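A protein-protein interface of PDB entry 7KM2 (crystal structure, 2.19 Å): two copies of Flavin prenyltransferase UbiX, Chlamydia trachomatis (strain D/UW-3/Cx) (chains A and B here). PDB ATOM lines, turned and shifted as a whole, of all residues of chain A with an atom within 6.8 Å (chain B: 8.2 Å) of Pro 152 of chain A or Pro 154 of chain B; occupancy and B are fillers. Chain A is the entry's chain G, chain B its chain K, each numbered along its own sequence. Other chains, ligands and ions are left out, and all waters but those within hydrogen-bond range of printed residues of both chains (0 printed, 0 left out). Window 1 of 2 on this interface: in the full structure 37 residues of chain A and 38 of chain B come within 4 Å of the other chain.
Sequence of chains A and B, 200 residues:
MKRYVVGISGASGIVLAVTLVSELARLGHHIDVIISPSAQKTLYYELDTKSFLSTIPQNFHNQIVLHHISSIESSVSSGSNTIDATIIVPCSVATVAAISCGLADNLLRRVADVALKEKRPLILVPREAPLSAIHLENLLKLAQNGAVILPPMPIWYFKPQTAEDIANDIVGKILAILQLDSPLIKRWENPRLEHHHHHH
Of the 18 printed residues of chain A, 12 touch a printed residue of chain B.
Along chain A the printed residues that touch a printed residue of chain B span positions 12 to 166.
Among the printed residues, no Asp or Glu carboxylate lies within 4 Å of a Lys or Arg side-chain nitrogen of the other chain.
Pro 151 of chain A touches Met 153 of chain B, and with the chains exchanged Met 153 of chain A touches Pro 151 of chain B.
Pro 152 of chain A touches Met 153 of chain B, and with the chains exchanged Met 153 of chain A touches Pro 152 of chain B.
Pro 152 of chain A touches Pro 154 of chain B, and with the chains exchanged Pro 154 of chain A touches Pro 152 of chain B.
Pro 154 of chain A touches its own counterpart, Pro 154 of chain B.
Positions printed for both chains: 127, 128, 151, 152, 153, 154, 156, 166 and 170.
The backbone NH (N) of Leu 150 of chain A sits at hydrogen-bond distance from the backbone carbonyl oxygen (O) of Leu 124 of chain A (2.9 Å).
Printed residues of chain B within 4 Å of Ser 12 of chain A: Trp 156 and Tyr 157.
Pro 152 of chain A touches just these residues of chain B: Met 153 and Pro 154.
Of the printed residues of chain B, Pro 154 of chain A touches Arg 127 (2.9 Å), Pro 152 (3.1 Å) and Pro 154 (3.7 Å).
Pro 154 of chain B touches just these residues of chain A: Arg 127 (2.9 Å), Pro 152 (3.3 Å) and Pro 154 (3.7 Å).
The nearest printed residue of chain B that does not touch Pro 152 of chain A is Trp 156 of chain B (4.1 Å).
The nearest printed residue of chain B that does not touch Pro 126 of chain A is Pro 151 of chain B (7.2 Å).
N of Trp 156 of chain B sits at hydrogen-bond distance from OG of Ser 12 of chain A (3.2 Å).
The guanidinium group (NE) of Arg 127 of chain A sits at hydrogen-bond distance from the backbone carbonyl oxygen (O) of Pro 154 of chain B (2.9 Å).
The guanidinium group of Arg 127 of chain B sits at hydrogen-bond distance from the backbone carbonyl oxygen of Met 153 of chain A, at 3.4 Å.
The backbone carbonyl oxygen (O) of Pro 154 of chain A lies within hydrogen-bond range of the guanidinium group (NE) of Arg 127 of chain B.
Among the printed residues, merely in contact across the chains: Pro 154 of chain A with Pro 152 of chain B (3.1 Å), Gly 13 of chain A with Trp 156 of chain B (3.2 Å), Met 153 of chain A with Glu 128 of chain B (3.2 Å), Pro 152 of chain A with Pro 154 of chain B (3.3 Å), Glu 128 of chain A with Met 153 of chain B (3.3 Å), Pro 126 of chain A with Met 153 of chain B (3.3 Å), Arg 127 of chain A with Ile 155 of chain B (3.5 Å), Ser 12 of chain A with Tyr 157 of chain B (3.5 Å), Arg 127 of chain A with Met 153 of chain B (3.5 Å), Pro 152 of chain A with Met 153 of chain B (3.6 Å), Pro 154 of chain A with Pro 154 of chain B (3.7 Å), Leu 150 of chain A with Ala 129 of chain B (3.7 Å), Leu 16 of chain A with Trp 156 of chain B (3.8 Å), Met 153 of chain A with Ala 129 of chain B (3.8 Å), Ile 166 of chain A with Ile 166 of chain B (3.8 Å), Ile 166 of chain A with Ala 163 of chain B (3.9 Å), Pro 151 of chain A with Ala 129 of chain B (3.9 Å), Pro 151 of chain A with Met 153 of chain B (3.9 Å), Met 153 of chain A with Pro 151 of chain B (3.99 Å) and Met 153 of chain A with Pro 152 of chain B (3.99 Å).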
ATOM      1  N   SER A  12       4.202  -8.920   4.281  1.00  0.00           N
ATOM      2  CA  SER A  12       3.086  -9.026   3.357  1.00  0.00           C
ATOM      3  C   SER A  12       3.188 -10.317   2.542  1.00  0.00           C
ATOM      4  O   SER A  12       4.286 -10.801   2.232  1.00  0.00           O
ATOM      5  CB  SER A  12       3.050  -7.814   2.432  1.00  0.00           C
ATOM      6  OG  SER A  12       1.935  -7.902   1.571  1.00  0.00           O
ATOM      7  N   GLY A  13       2.028 -10.890   2.227  1.00  0.00           N
ATOM      8  CA  GLY A  13       1.957 -12.086   1.406  1.00  0.00           C
ATOM      9  C   GLY A  13       1.626 -13.359   2.145  1.00  0.00           C
ATOM     10  O   GLY A  13       2.149 -14.431   1.819  1.00  0.00           O
ATOM     11  N   LEU A  16       0.767 -16.647   0.556  1.00  0.00           N
ATOM     12  CA  LEU A  16       1.777 -17.612   0.143  1.00  0.00           C
ATOM     13  C   LEU A  16       1.874 -18.772   1.135  1.00  0.00           C
ATOM     14  O   LEU A  16       1.958 -19.940   0.731  1.00  0.00           O
ATOM     15  CB  LEU A  16       3.131 -16.925  -0.021  1.00  0.00           C
ATOM     16  CG  LEU A  16       3.250 -15.796  -1.056  1.00  0.00           C
ATOM     17  CD1 LEU A  16       4.631 -15.145  -0.979  1.00  0.00           C
ATOM     18  CD2 LEU A  16       2.958 -16.285  -2.480  1.00  0.00           C
ATOM     19  N   VAL A  89       7.886 -18.323   5.486  1.00  0.00           N
ATOM     20  CA  VAL A  89       7.164 -17.630   4.426  1.00  0.00           C
ATOM     21  C   VAL A  89       5.882 -17.004   4.963  1.00  0.00           C
ATOM     22  O   VAL A  89       5.135 -17.659   5.700  1.00  0.00           O
ATOM     23  CB  VAL A  89       6.863 -18.589   3.250  1.00  0.00           C
ATOM     24  CG1 VAL A  89       6.052 -19.804   3.723  1.00  0.00           C
ATOM     25  CG2 VAL A  89       6.155 -17.846   2.109  1.00  0.00           C
ATOM     26  N   PRO A  90       5.663 -15.705   4.685  1.00  0.00           N
ATOM     27  CA  PRO A  90       6.672 -14.761   4.192  1.00  0.00           C
ATOM     28  C   PRO A  90       7.667 -14.453   5.310  1.00  0.00           C
ATOM     29  O   PRO A  90       7.374 -14.708   6.469  1.00  0.00           O
ATOM     30  CB  PRO A  90       5.869 -13.502   3.833  1.00  0.00           C
ATOM     31  CG  PRO A  90       4.449 -13.740   4.282  1.00  0.00           C
ATOM     32  CD  PRO A  90       4.417 -15.022   5.077  1.00  0.00           C
ATOM     33  N   LEU A 124      13.871 -19.283   2.853  1.00  0.00           N
ATOM     34  CA  LEU A 124      13.363 -18.007   3.328  1.00  0.00           C
ATOM     35  C   LEU A 124      12.716 -17.306   2.151  1.00  0.00           C
ATOM     36  O   LEU A 124      13.291 -17.280   1.053  1.00  0.00           O
ATOM     37  CB  LEU A 124      14.488 -17.151   3.916  1.00  0.00           C
ATOM     38  CG  LEU A 124      15.358 -17.821   4.995  1.00  0.00           C
ATOM     39  CD1 LEU A 124      16.457 -16.883   5.453  1.00  0.00           C
ATOM     40  CD2 LEU A 124      14.534 -18.334   6.198  1.00  0.00           C
ATOM     41  N   VAL A 125      11.521 -16.768   2.371  1.00  0.00           N
ATOM     42  CA  VAL A 125      10.808 -16.046   1.322  1.00  0.00           C
ATOM     43  C   VAL A 125      10.732 -14.592   1.760  1.00  0.00           C
ATOM     44  O   VAL A 125       9.675 -14.109   2.203  1.00  0.00           O
ATOM     45  CB  VAL A 125       9.429 -16.662   1.050  1.00  0.00           C
ATOM     46  CG1 VAL A 125       8.754 -15.966  -0.122  1.00  0.00           C
ATOM     47  CG2 VAL A 125       9.582 -18.155   0.755  1.00  0.00           C
ATOM     48  N   PRO A 126      11.831 -13.860   1.645  1.00  0.00           N
ATOM     49  CA  PRO A 126      11.866 -12.499   2.175  1.00  0.00           C
ATOM     50  C   PRO A 126      11.151 -11.541   1.248  1.00  0.00           C
ATOM     51  O   PRO A 126      11.330 -11.563   0.029  1.00  0.00           O
ATOM     52  CB  PRO A 126      13.366 -12.192   2.243  1.00  0.00           C
ATOM     53  CG  PRO A 126      13.928 -12.948   1.075  1.00  0.00           C
ATOM     54  CD  PRO A 126      13.077 -14.210   0.940  1.00  0.00           C
ATOM     55  N   ARG A 127      10.337 -10.683   1.848  1.00  0.00           N
ATOM     56  CA  ARG A 127       9.542  -9.715   1.113  1.00  0.00           C
ATOM     57  C   ARG A 127       9.801  -8.338   1.708  1.00  0.00           C
ATOM     58  O   ARG A 127       9.490  -8.095   2.880  1.00  0.00           O
ATOM     59  CB  ARG A 127       8.066 -10.072   1.184  1.00  0.00           C
ATOM     60  CG  ARG A 127       7.272  -9.341   0.155  1.00  0.00           C
ATOM     61  CD  ARG A 127       6.111  -8.576   0.742  1.00  0.00           C
ATOM     62  NE  ARG A 127       5.712  -7.597  -0.254  1.00  0.00           N
ATOM     63  CZ  ARG A 127       6.101  -6.327  -0.250  1.00  0.00           C
ATOM     64  NH1 ARG A 127       6.859  -5.861   0.739  1.00  0.00           N
ATOM     65  NH2 ARG A 127       5.706  -5.523  -1.230  1.00  0.00           N
ATOM     66  N   GLU A 128      10.398  -7.456   0.917  1.00  0.00           N
ATOM     67  CA  GLU A 128      10.666  -6.085   1.330  1.00  0.00           C
ATOM     68  C   GLU A 128      11.213  -5.364   0.112  1.00  0.00           C
ATOM     69  O   GLU A 128      12.023  -5.928  -0.626  1.00  0.00           O
ATOM     70  CB  GLU A 128      11.682  -6.005   2.489  1.00  0.00           C
ATOM     71  CG  GLU A 128      12.070  -4.562   2.947  1.00  0.00           C
ATOM     72  CD  GLU A 128      10.867  -3.756   3.468  1.00  0.00           C
ATOM     73  OE1 GLU A 128      10.782  -3.538   4.702  1.00  0.00           O
ATOM     74  OE2 GLU A 128      10.002  -3.352   2.644  1.00  0.00           O
ATOM     75  N   LEU A 150      14.711 -17.059  -1.451  1.00  0.00           N
ATOM     76  CA  LEU A 150      13.695 -17.167  -2.490  1.00  0.00           C
ATOM     77  C   LEU A 150      12.687 -16.033  -2.336  1.00  0.00           C
ATOM     78  O   LEU A 150      11.597 -16.231  -1.779  1.00  0.00           O
ATOM     79  CB  LEU A 150      12.992 -18.520  -2.416  1.00  0.00           C
ATOM     80  CG  LEU A 150      12.050 -18.786  -3.590  1.00  0.00           C
ATOM     81  CD1 LEU A 150      12.859 -19.033  -4.837  1.00  0.00           C
ATOM     82  CD2 LEU A 150      11.174 -19.979  -3.277  1.00  0.00           C
ATOM     83  N   PRO A 151      13.008 -14.828  -2.810  1.00  0.00           N
ATOM     84  CA  PRO A 151      12.044 -13.742  -2.725  1.00  0.00           C
ATOM     85  C   PRO A 151      10.845 -14.064  -3.594  1.00  0.00           C
ATOM     86  O   PRO A 151      10.968 -14.781  -4.601  1.00  0.00           O
ATOM     87  CB  PRO A 151      12.820 -12.532  -3.279  1.00  0.00           C
ATOM     88  CG  PRO A 151      14.230 -13.019  -3.525  1.00  0.00           C
ATOM     89  CD  PRO A 151      14.128 -14.488  -3.698  1.00  0.00           C
ATOM     90  N   PRO A 152       9.680 -13.566  -3.256  1.00  0.00           N
ATOM     91  CA  PRO A 152       8.477 -13.949  -4.020  1.00  0.00           C
ATOM     92  C   PRO A 152       8.362 -13.163  -5.323  1.00  0.00           C
ATOM     93  O   PRO A 152       7.549 -12.248  -5.496  1.00  0.00           O
ATOM     94  CB  PRO A 152       7.349 -13.666  -3.018  1.00  0.00           C
ATOM     95  CG  PRO A 152       7.896 -12.572  -2.129  1.00  0.00           C
ATOM     96  CD  PRO A 152       9.385 -12.688  -2.111  1.00  0.00           C
ATOM     97  N   MET A 153       9.210 -13.541  -6.270  1.00  0.00           N
ATOM     98  CA  MET A 153       9.283 -12.895  -7.574  1.00  0.00           C
ATOM     99  C   MET A 153       8.216 -13.469  -8.500  1.00  0.00           C
ATOM    100  O   MET A 153       8.219 -14.676  -8.745  1.00  0.00           O
ATOM    101  CB  MET A 153      10.655 -13.131  -8.195  1.00  0.00           C
ATOM    102  CG  MET A 153      11.850 -12.847  -7.306  1.00  0.00           C
ATOM    103  SD  MET A 153      12.279 -11.106  -7.445  1.00  0.00           S
ATOM    104  CE  MET A 153      13.963 -11.071  -6.801  1.00  0.00           C
ATOM    105  N   PRO A 154       7.315 -12.653  -9.052  1.00  0.00           N
ATOM    106  CA  PRO A 154       6.329 -13.194 -10.000  1.00  0.00           C
ATOM    107  C   PRO A 154       6.985 -13.764 -11.254  1.00  0.00           C
ATOM    108  O   PRO A 154       7.954 -13.217 -11.793  1.00  0.00           O
ATOM    109  CB  PRO A 154       5.446 -11.984 -10.325  1.00  0.00           C
ATOM    110  CG  PRO A 154       5.633 -11.051  -9.163  1.00  0.00           C
ATOM    111  CD  PRO A 154       7.062 -11.236  -8.754  1.00  0.00           C
ATOM    112  N   TRP A 156       6.412 -14.126 -14.741  1.00  0.00           N
ATOM    113  CA  TRP A 156       5.528 -13.604 -15.774  1.00  0.00           C
ATOM    114  C   TRP A 156       5.533 -14.426 -17.056  1.00  0.00           C
ATOM    115  O   TRP A 156       4.569 -14.332 -17.821  1.00  0.00           O
ATOM    116  CB  TRP A 156       5.885 -12.158 -16.097  1.00  0.00           C
ATOM    117  CG  TRP A 156       5.245 -11.191 -15.159  1.00  0.00           C
ATOM    118  CD1 TRP A 156       3.929 -10.815 -15.141  1.00  0.00           C
ATOM    119  CD2 TRP A 156       5.882 -10.478 -14.088  1.00  0.00           C
ATOM    120  NE1 TRP A 156       3.708  -9.914 -14.135  1.00  0.00           N
ATOM    121  CE2 TRP A 156       4.884  -9.692 -13.466  1.00  0.00           C
ATOM    122  CE3 TRP A 156       7.188 -10.441 -13.584  1.00  0.00           C
ATOM    123  CZ2 TRP A 156       5.154  -8.871 -12.376  1.00  0.00           C
ATOM    124  CZ3 TRP A 156       7.461  -9.612 -12.492  1.00  0.00           C
ATOM    125  CH2 TRP A 156       6.447  -8.844 -11.899  1.00  0.00           C
ATOM    126  N   ILE A 166      -0.421 -15.714  -9.700  1.00  0.00           N
ATOM    127  CA  ILE A 166       0.936 -15.316  -9.344  1.00  0.00           C
ATOM    128  C   ILE A 166       1.361 -15.988  -8.044  1.00  0.00           C
ATOM    129  O   ILE A 166       2.490 -16.480  -7.928  1.00  0.00           O
ATOM    130  CB  ILE A 166       1.016 -13.781  -9.273  1.00  0.00           C
ATOM    131  CG1 ILE A 166       0.923 -13.222 -10.700  1.00  0.00           C
ATOM    132  CG2 ILE A 166       2.273 -13.320  -8.542  1.00  0.00           C
ATOM    133  CD1 ILE A 166       0.900 -11.716 -10.793  1.00  0.00           C
ATOM    134  N   ILE A 170       4.501 -18.860  -7.548  1.00  0.00           N
ATOM    135  CA  ILE A 170       5.527 -18.637  -6.534  1.00  0.00           C
ATOM    136  C   ILE A 170       5.591 -19.824  -5.571  1.00  0.00           C
ATOM    137  O   ILE A 170       6.672 -20.348  -5.282  1.00  0.00           O
ATOM    138  CB  ILE A 170       5.260 -17.305  -5.808  1.00  0.00           C
ATOM    139  CG1 ILE A 170       5.606 -16.132  -6.721  1.00  0.00           C
ATOM    140  CG2 ILE A 170       6.059 -17.194  -4.524  1.00  0.00           C
ATOM    141  CD1 ILE A 170       5.297 -14.801  -6.092  1.00  0.00           C
ATOM    142  N   ARG B 127      15.058  -9.222 -11.104  1.00  0.00           N
ATOM    143  CA  ARG B 127      14.135 -10.342 -11.025  1.00  0.00           C
ATOM    144  C   ARG B 127      14.936 -11.631 -11.201  1.00  0.00           C
ATOM    145  O   ARG B 127      15.488 -11.880 -12.277  1.00  0.00           O
ATOM    146  CB  ARG B 127      13.040 -10.202 -12.079  1.00  0.00           C
ATOM    147  CG  ARG B 127      11.824 -11.043 -11.791  1.00  0.00           C
ATOM    148  CD  ARG B 127      11.714 -12.191 -12.754  1.00  0.00           C
ATOM    149  NE  ARG B 127      10.802 -13.204 -12.238  1.00  0.00           N
ATOM    150  CZ  ARG B 127      11.166 -14.436 -11.892  1.00  0.00           C
ATOM    151  NH1 ARG B 127      12.427 -14.829 -12.030  1.00  0.00           N
ATOM    152  NH2 ARG B 127      10.261 -15.282 -11.420  1.00  0.00           N
ATOM    153  N   GLU B 128      15.029 -12.423 -10.135  1.00  0.00           N
ATOM    154  CA  GLU B 128      15.644 -13.745 -10.170  1.00  0.00           C
ATOM    155  C   GLU B 128      15.330 -14.442  -8.856  1.00  0.00           C
ATOM    156  O   GLU B 128      15.286 -13.796  -7.812  1.00  0.00           O
ATOM    157  CB  GLU B 128      17.166 -13.670 -10.379  1.00  0.00           C
ATOM    158  CG  GLU B 128      17.900 -15.028 -10.470  1.00  0.00           C
ATOM    159  CD  GLU B 128      17.415 -15.894 -11.628  1.00  0.00           C
ATOM    160  OE1 GLU B 128      16.389 -16.592 -11.458  1.00  0.00           O
ATOM    161  OE2 GLU B 128      18.044 -15.871 -12.713  1.00  0.00           O
ATOM    162  N   ALA B 129      15.112 -15.752  -8.913  1.00  0.00           N
ATOM    163  CA  ALA B 129      14.802 -16.532  -7.725  1.00  0.00           C
ATOM    164  C   ALA B 129      15.096 -18.005  -7.963  1.00  0.00           C
ATOM    165  O   ALA B 129      14.710 -18.556  -8.987  1.00  0.00           O
ATOM    166  CB  ALA B 129      13.348 -16.334  -7.321  1.00  0.00           C
ATOM    167  N   PRO B 151      13.378  -5.059  -5.963  1.00  0.00           N
ATOM    168  CA  PRO B 151      12.841  -6.285  -6.545  1.00  0.00           C
ATOM    169  C   PRO B 151      11.338  -6.178  -6.703  1.00  0.00           C
ATOM    170  O   PRO B 151      10.656  -5.537  -5.880  1.00  0.00           O
ATOM    171  CB  PRO B 151      13.220  -7.367  -5.523  1.00  0.00           C
ATOM    172  CG  PRO B 151      14.063  -6.705  -4.481  1.00  0.00           C
ATOM    173  CD  PRO B 151      13.808  -5.239  -4.567  1.00  0.00           C
ATOM    174  N   PRO B 152      10.772  -6.781  -7.754  1.00  0.00           N
ATOM    175  CA  PRO B 152       9.317  -6.643  -7.964  1.00  0.00           C
ATOM    176  C   PRO B 152       8.520  -7.563  -7.038  1.00  0.00           C
ATOM    177  O   PRO B 152       7.992  -8.601  -7.417  1.00  0.00           O
ATOM    178  CB  PRO B 152       9.165  -6.992  -9.448  1.00  0.00           C
ATOM    179  CG  PRO B 152      10.268  -7.953  -9.721  1.00  0.00           C
ATOM    180  CD  PRO B 152      11.435  -7.476  -8.870  1.00  0.00           C
ATOM    181  N   MET B 153       8.457  -7.161  -5.770  1.00  0.00           N
ATOM    182  CA  MET B 153       7.674  -7.868  -4.759  1.00  0.00           C
ATOM    183  C   MET B 153       6.216  -7.433  -4.828  1.00  0.00           C
ATOM    184  O   MET B 153       5.933  -6.245  -4.664  1.00  0.00           O
ATOM    185  CB  MET B 153       8.202  -7.555  -3.366  1.00  0.00           C
ATOM    186  CG  MET B 153       9.694  -7.557  -3.210  1.00  0.00           C
ATOM    187  SD  MET B 153      10.190  -9.216  -2.786  1.00  0.00           S
ATOM    188  CE  MET B 153      11.792  -8.947  -1.999  1.00  0.00           C
ATOM    189  N   PRO B 154       5.267  -8.343  -5.034  1.00  0.00           N
ATOM    190  CA  PRO B 154       3.852  -7.954  -4.970  1.00  0.00           C
ATOM    191  C   PRO B 154       3.483  -7.365  -3.610  1.00  0.00           C
ATOM    192  O   PRO B 154       3.997  -7.770  -2.564  1.00  0.00           O
ATOM    193  CB  PRO B 154       3.113  -9.272  -5.215  1.00  0.00           C
ATOM    194  CG  PRO B 154       4.117 -10.142  -5.920  1.00  0.00           C
ATOM    195  CD  PRO B 154       5.440  -9.773  -5.338  1.00  0.00           C
ATOM    196  N   ILE B 155       2.552  -6.425  -3.633  1.00  0.00           N
ATOM    197  CA  ILE B 155       2.040  -5.771  -2.433  1.00  0.00           C
ATOM    198  C   ILE B 155       0.656  -6.346  -2.175  1.00  0.00           C
ATOM    199  O   ILE B 155      -0.343  -5.862  -2.725  1.00  0.00           O
ATOM    200  CB  ILE B 155       1.995  -4.245  -2.594  1.00  0.00           C
ATOM    201  CG1 ILE B 155       3.351  -3.724  -3.069  1.00  0.00           C
ATOM    202  CG2 ILE B 155       1.593  -3.576  -1.285  1.00  0.00           C
ATOM    203  CD1 ILE B 155       3.250  -2.756  -4.214  1.00  0.00           C
ATOM    204  N   TRP B 156       0.577  -7.364  -1.312  1.00  0.00           N
ATOM    205  CA  TRP B 156      -0.694  -8.048  -1.104  1.00  0.00           C
ATOM    206  C   TRP B 156      -1.672  -7.275  -0.232  1.00  0.00           C
ATOM    207  O   TRP B 156      -2.885  -7.512  -0.344  1.00  0.00           O
ATOM    208  CB  TRP B 156      -0.458  -9.438  -0.515  1.00  0.00           C
ATOM    209  CG  TRP B 156      -0.046 -10.415  -1.579  1.00  0.00           C
ATOM    210  CD1 TRP B 156      -0.864 -11.038  -2.482  1.00  0.00           C
ATOM    211  CD2 TRP B 156       1.286 -10.853  -1.876  1.00  0.00           C
ATOM    212  NE1 TRP B 156      -0.125 -11.851  -3.314  1.00  0.00           N
ATOM    213  CE2 TRP B 156       1.196 -11.757  -2.962  1.00  0.00           C
ATOM    214  CE3 TRP B 156       2.542 -10.571  -1.332  1.00  0.00           C
ATOM    215  CZ2 TRP B 156       2.317 -12.383  -3.504  1.00  0.00           C
ATOM    216  CZ3 TRP B 156       3.654 -11.210  -1.857  1.00  0.00           C
ATOM    217  CH2 TRP B 156       3.536 -12.098  -2.944  1.00  0.00           C
ATOM    218  N   TYR B 157      -1.209  -6.350   0.611  1.00  0.00           N
ATOM    219  CA  TYR B 157      -2.167  -5.634   1.446  1.00  0.00           C
ATOM    220  C   TYR B 157      -2.919  -4.541   0.693  1.00  0.00           C
ATOM    221  O   TYR B 157      -3.722  -3.833   1.307  1.00  0.00           O
ATOM    222  CB  TYR B 157      -1.496  -5.050   2.699  1.00  0.00           C
ATOM    223  CG  TYR B 157      -0.302  -4.178   2.439  1.00  0.00           C
ATOM    224  CD1 TYR B 157      -0.457  -2.851   2.072  1.00  0.00           C
ATOM    225  CD2 TYR B 157       0.989  -4.681   2.569  1.00  0.00           C
ATOM    226  CE1 TYR B 157       0.644  -2.046   1.827  1.00  0.00           C
ATOM    227  CE2 TYR B 157       2.096  -3.888   2.331  1.00  0.00           C
ATOM    228  CZ  TYR B 157       1.918  -2.570   1.959  1.00  0.00           C
ATOM    229  OH  TYR B 157       3.007  -1.773   1.715  1.00  0.00           O
ATOM    230  N   PHE B 158      -2.692  -4.380  -0.609  1.00  0.00           N
ATOM    231  CA  PHE B 158      -3.631  -3.650  -1.443  1.00  0.00           C
ATOM    232  C   PHE B 158      -4.709  -4.559  -2.002  1.00  0.00           C
ATOM    233  O   PHE B 158      -5.548  -4.096  -2.786  1.00  0.00           O
ATOM    234  CB  PHE B 158      -2.905  -2.933  -2.584  1.00  0.00           C
ATOM    235  CG  PHE B 158      -2.037  -1.798  -2.121  1.00  0.00           C
ATOM    236  CD1 PHE B 158      -2.389  -1.054  -1.008  1.00  0.00           C
ATOM    237  CD2 PHE B 158      -0.872  -1.479  -2.793  1.00  0.00           C
ATOM    238  CE1 PHE B 158      -1.600  -0.008  -0.575  1.00  0.00           C
ATOM    239  CE2 PHE B 158      -0.074  -0.432  -2.360  1.00  0.00           C
ATOM    240  CZ  PHE B 158      -0.437   0.298  -1.245  1.00  0.00           C
ATOM    241  N   PRO B 160      -4.849  -7.158  -4.255  1.00  0.00           N
ATOM    242  CA  PRO B 160      -4.989  -7.198  -5.712  1.00  0.00           C
ATOM    243  C   PRO B 160      -5.826  -8.387  -6.140  1.00  0.00           C
ATOM    244  O   PRO B 160      -5.828  -9.447  -5.506  1.00  0.00           O
ATOM    245  CB  PRO B 160      -3.541  -7.323  -6.194  1.00  0.00           C
ATOM    246  CG  PRO B 160      -2.849  -8.035  -5.079  1.00  0.00           C
ATOM    247  CD  PRO B 160      -3.543  -7.668  -3.800  1.00  0.00           C
ATOM    248  N   ALA B 163      -3.579 -10.086 -12.251  1.00  0.00           N
ATOM    249  CA  ALA B 163      -2.145  -9.940 -12.485  1.00  0.00           C
ATOM    250  C   ALA B 163      -1.786  -8.475 -12.716  1.00  0.00           C
ATOM    251  O   ALA B 163      -0.811  -7.963 -12.147  1.00  0.00           O
ATOM    252  CB  ALA B 163      -1.719 -10.800 -13.678  1.00  0.00           C
ATOM    253  N   ASP B 165      -3.152  -5.841 -11.586  1.00  0.00           N
ATOM    254  CA  ASP B 165      -3.127  -5.125 -10.313  1.00  0.00           C
ATOM    255  C   ASP B 165      -1.755  -5.208  -9.664  1.00  0.00           C
ATOM    256  O   ASP B 165      -1.225  -4.204  -9.180  1.00  0.00           O
ATOM    257  CB  ASP B 165      -4.188  -5.689  -9.361  1.00  0.00           C
ATOM    258  CG  ASP B 165      -5.596  -5.282  -9.741  1.00  0.00           C
ATOM    259  OD1 ASP B 165      -5.776  -4.142 -10.218  1.00  0.00           O
ATOM    260  OD2 ASP B 165      -6.522  -6.105  -9.558  1.00  0.00           O
ATOM    261  N   ILE B 166      -1.165  -6.402  -9.641  1.00  0.00           N
ATOM    262  CA  ILE B 166       0.139  -6.552  -8.999  1.00  0.00           C
ATOM    263  C   ILE B 166       1.205  -5.784  -9.770  1.00  0.00           C
ATOM    264  O   ILE B 166       2.036  -5.089  -9.173  1.00  0.00           O
ATOM    265  CB  ILE B 166       0.484  -8.040  -8.836  1.00  0.00           C
ATOM    266  CG1 ILE B 166      -0.330  -8.609  -7.665  1.00  0.00           C
ATOM    267  CG2 ILE B 166       1.996  -8.226  -8.620  1.00  0.00           C
ATOM    268  CD1 ILE B 166      -0.354 -10.100  -7.591  1.00  0.00           C
ATOM    269  N   ALA B 167       1.175  -5.856 -11.102  1.00  0.00           N
ATOM    270  CA  ALA B 167       2.118  -5.074 -11.899  1.00  0.00           C
ATOM    271  C   ALA B 167       1.944  -3.582 -11.640  1.00  0.00           C
ATOM    272  O   ALA B 167       2.925  -2.860 -11.406  1.00  0.00           O
ATOM    273  CB  ALA B 167       1.951  -5.378 -13.382  1.00  0.00           C
ATOM    274  N   ASP B 169       0.744  -1.922  -9.026  1.00  0.00           N
ATOM    275  CA  ASP B 169       1.225  -1.473  -7.722  1.00  0.00           C
ATOM    276  C   ASP B 169       2.749  -1.507  -7.638  1.00  0.00           C
ATOM    277  O   ASP B 169       3.351  -0.663  -6.963  1.00  0.00           O
ATOM    278  CB  ASP B 169       0.616  -2.320  -6.600  1.00  0.00           C
ATOM    279  CG  ASP B 169      -0.879  -2.128  -6.458  1.00  0.00           C
ATOM    280  OD1 ASP B 169      -1.383  -1.043  -6.830  1.00  0.00           O
ATOM    281  OD2 ASP B 169      -1.551  -3.060  -5.964  1.00  0.00           O
ATOM    282  N   ILE B 170       3.393  -2.461  -8.312  1.00  0.00           N
ATOM    283  CA  ILE B 170       4.852  -2.469  -8.350  1.00  0.00           C
ATOM    284  C   ILE B 170       5.372  -1.212  -9.037  1.00  0.00           C
ATOM    285  O   ILE B 170       6.302  -0.555  -8.545  1.00  0.00           O
ATOM    286  CB  ILE B 170       5.351  -3.755  -9.033  1.00  0.00           C
ATOM    287  CG1 ILE B 170       5.162  -4.950  -8.104  1.00  0.00           C
ATOM    288  CG2 ILE B 170       6.804  -3.624  -9.450  1.00  0.00           C
ATOM    289  CD1 ILE B 170       5.270  -6.290  -8.810  1.00  0.00           C
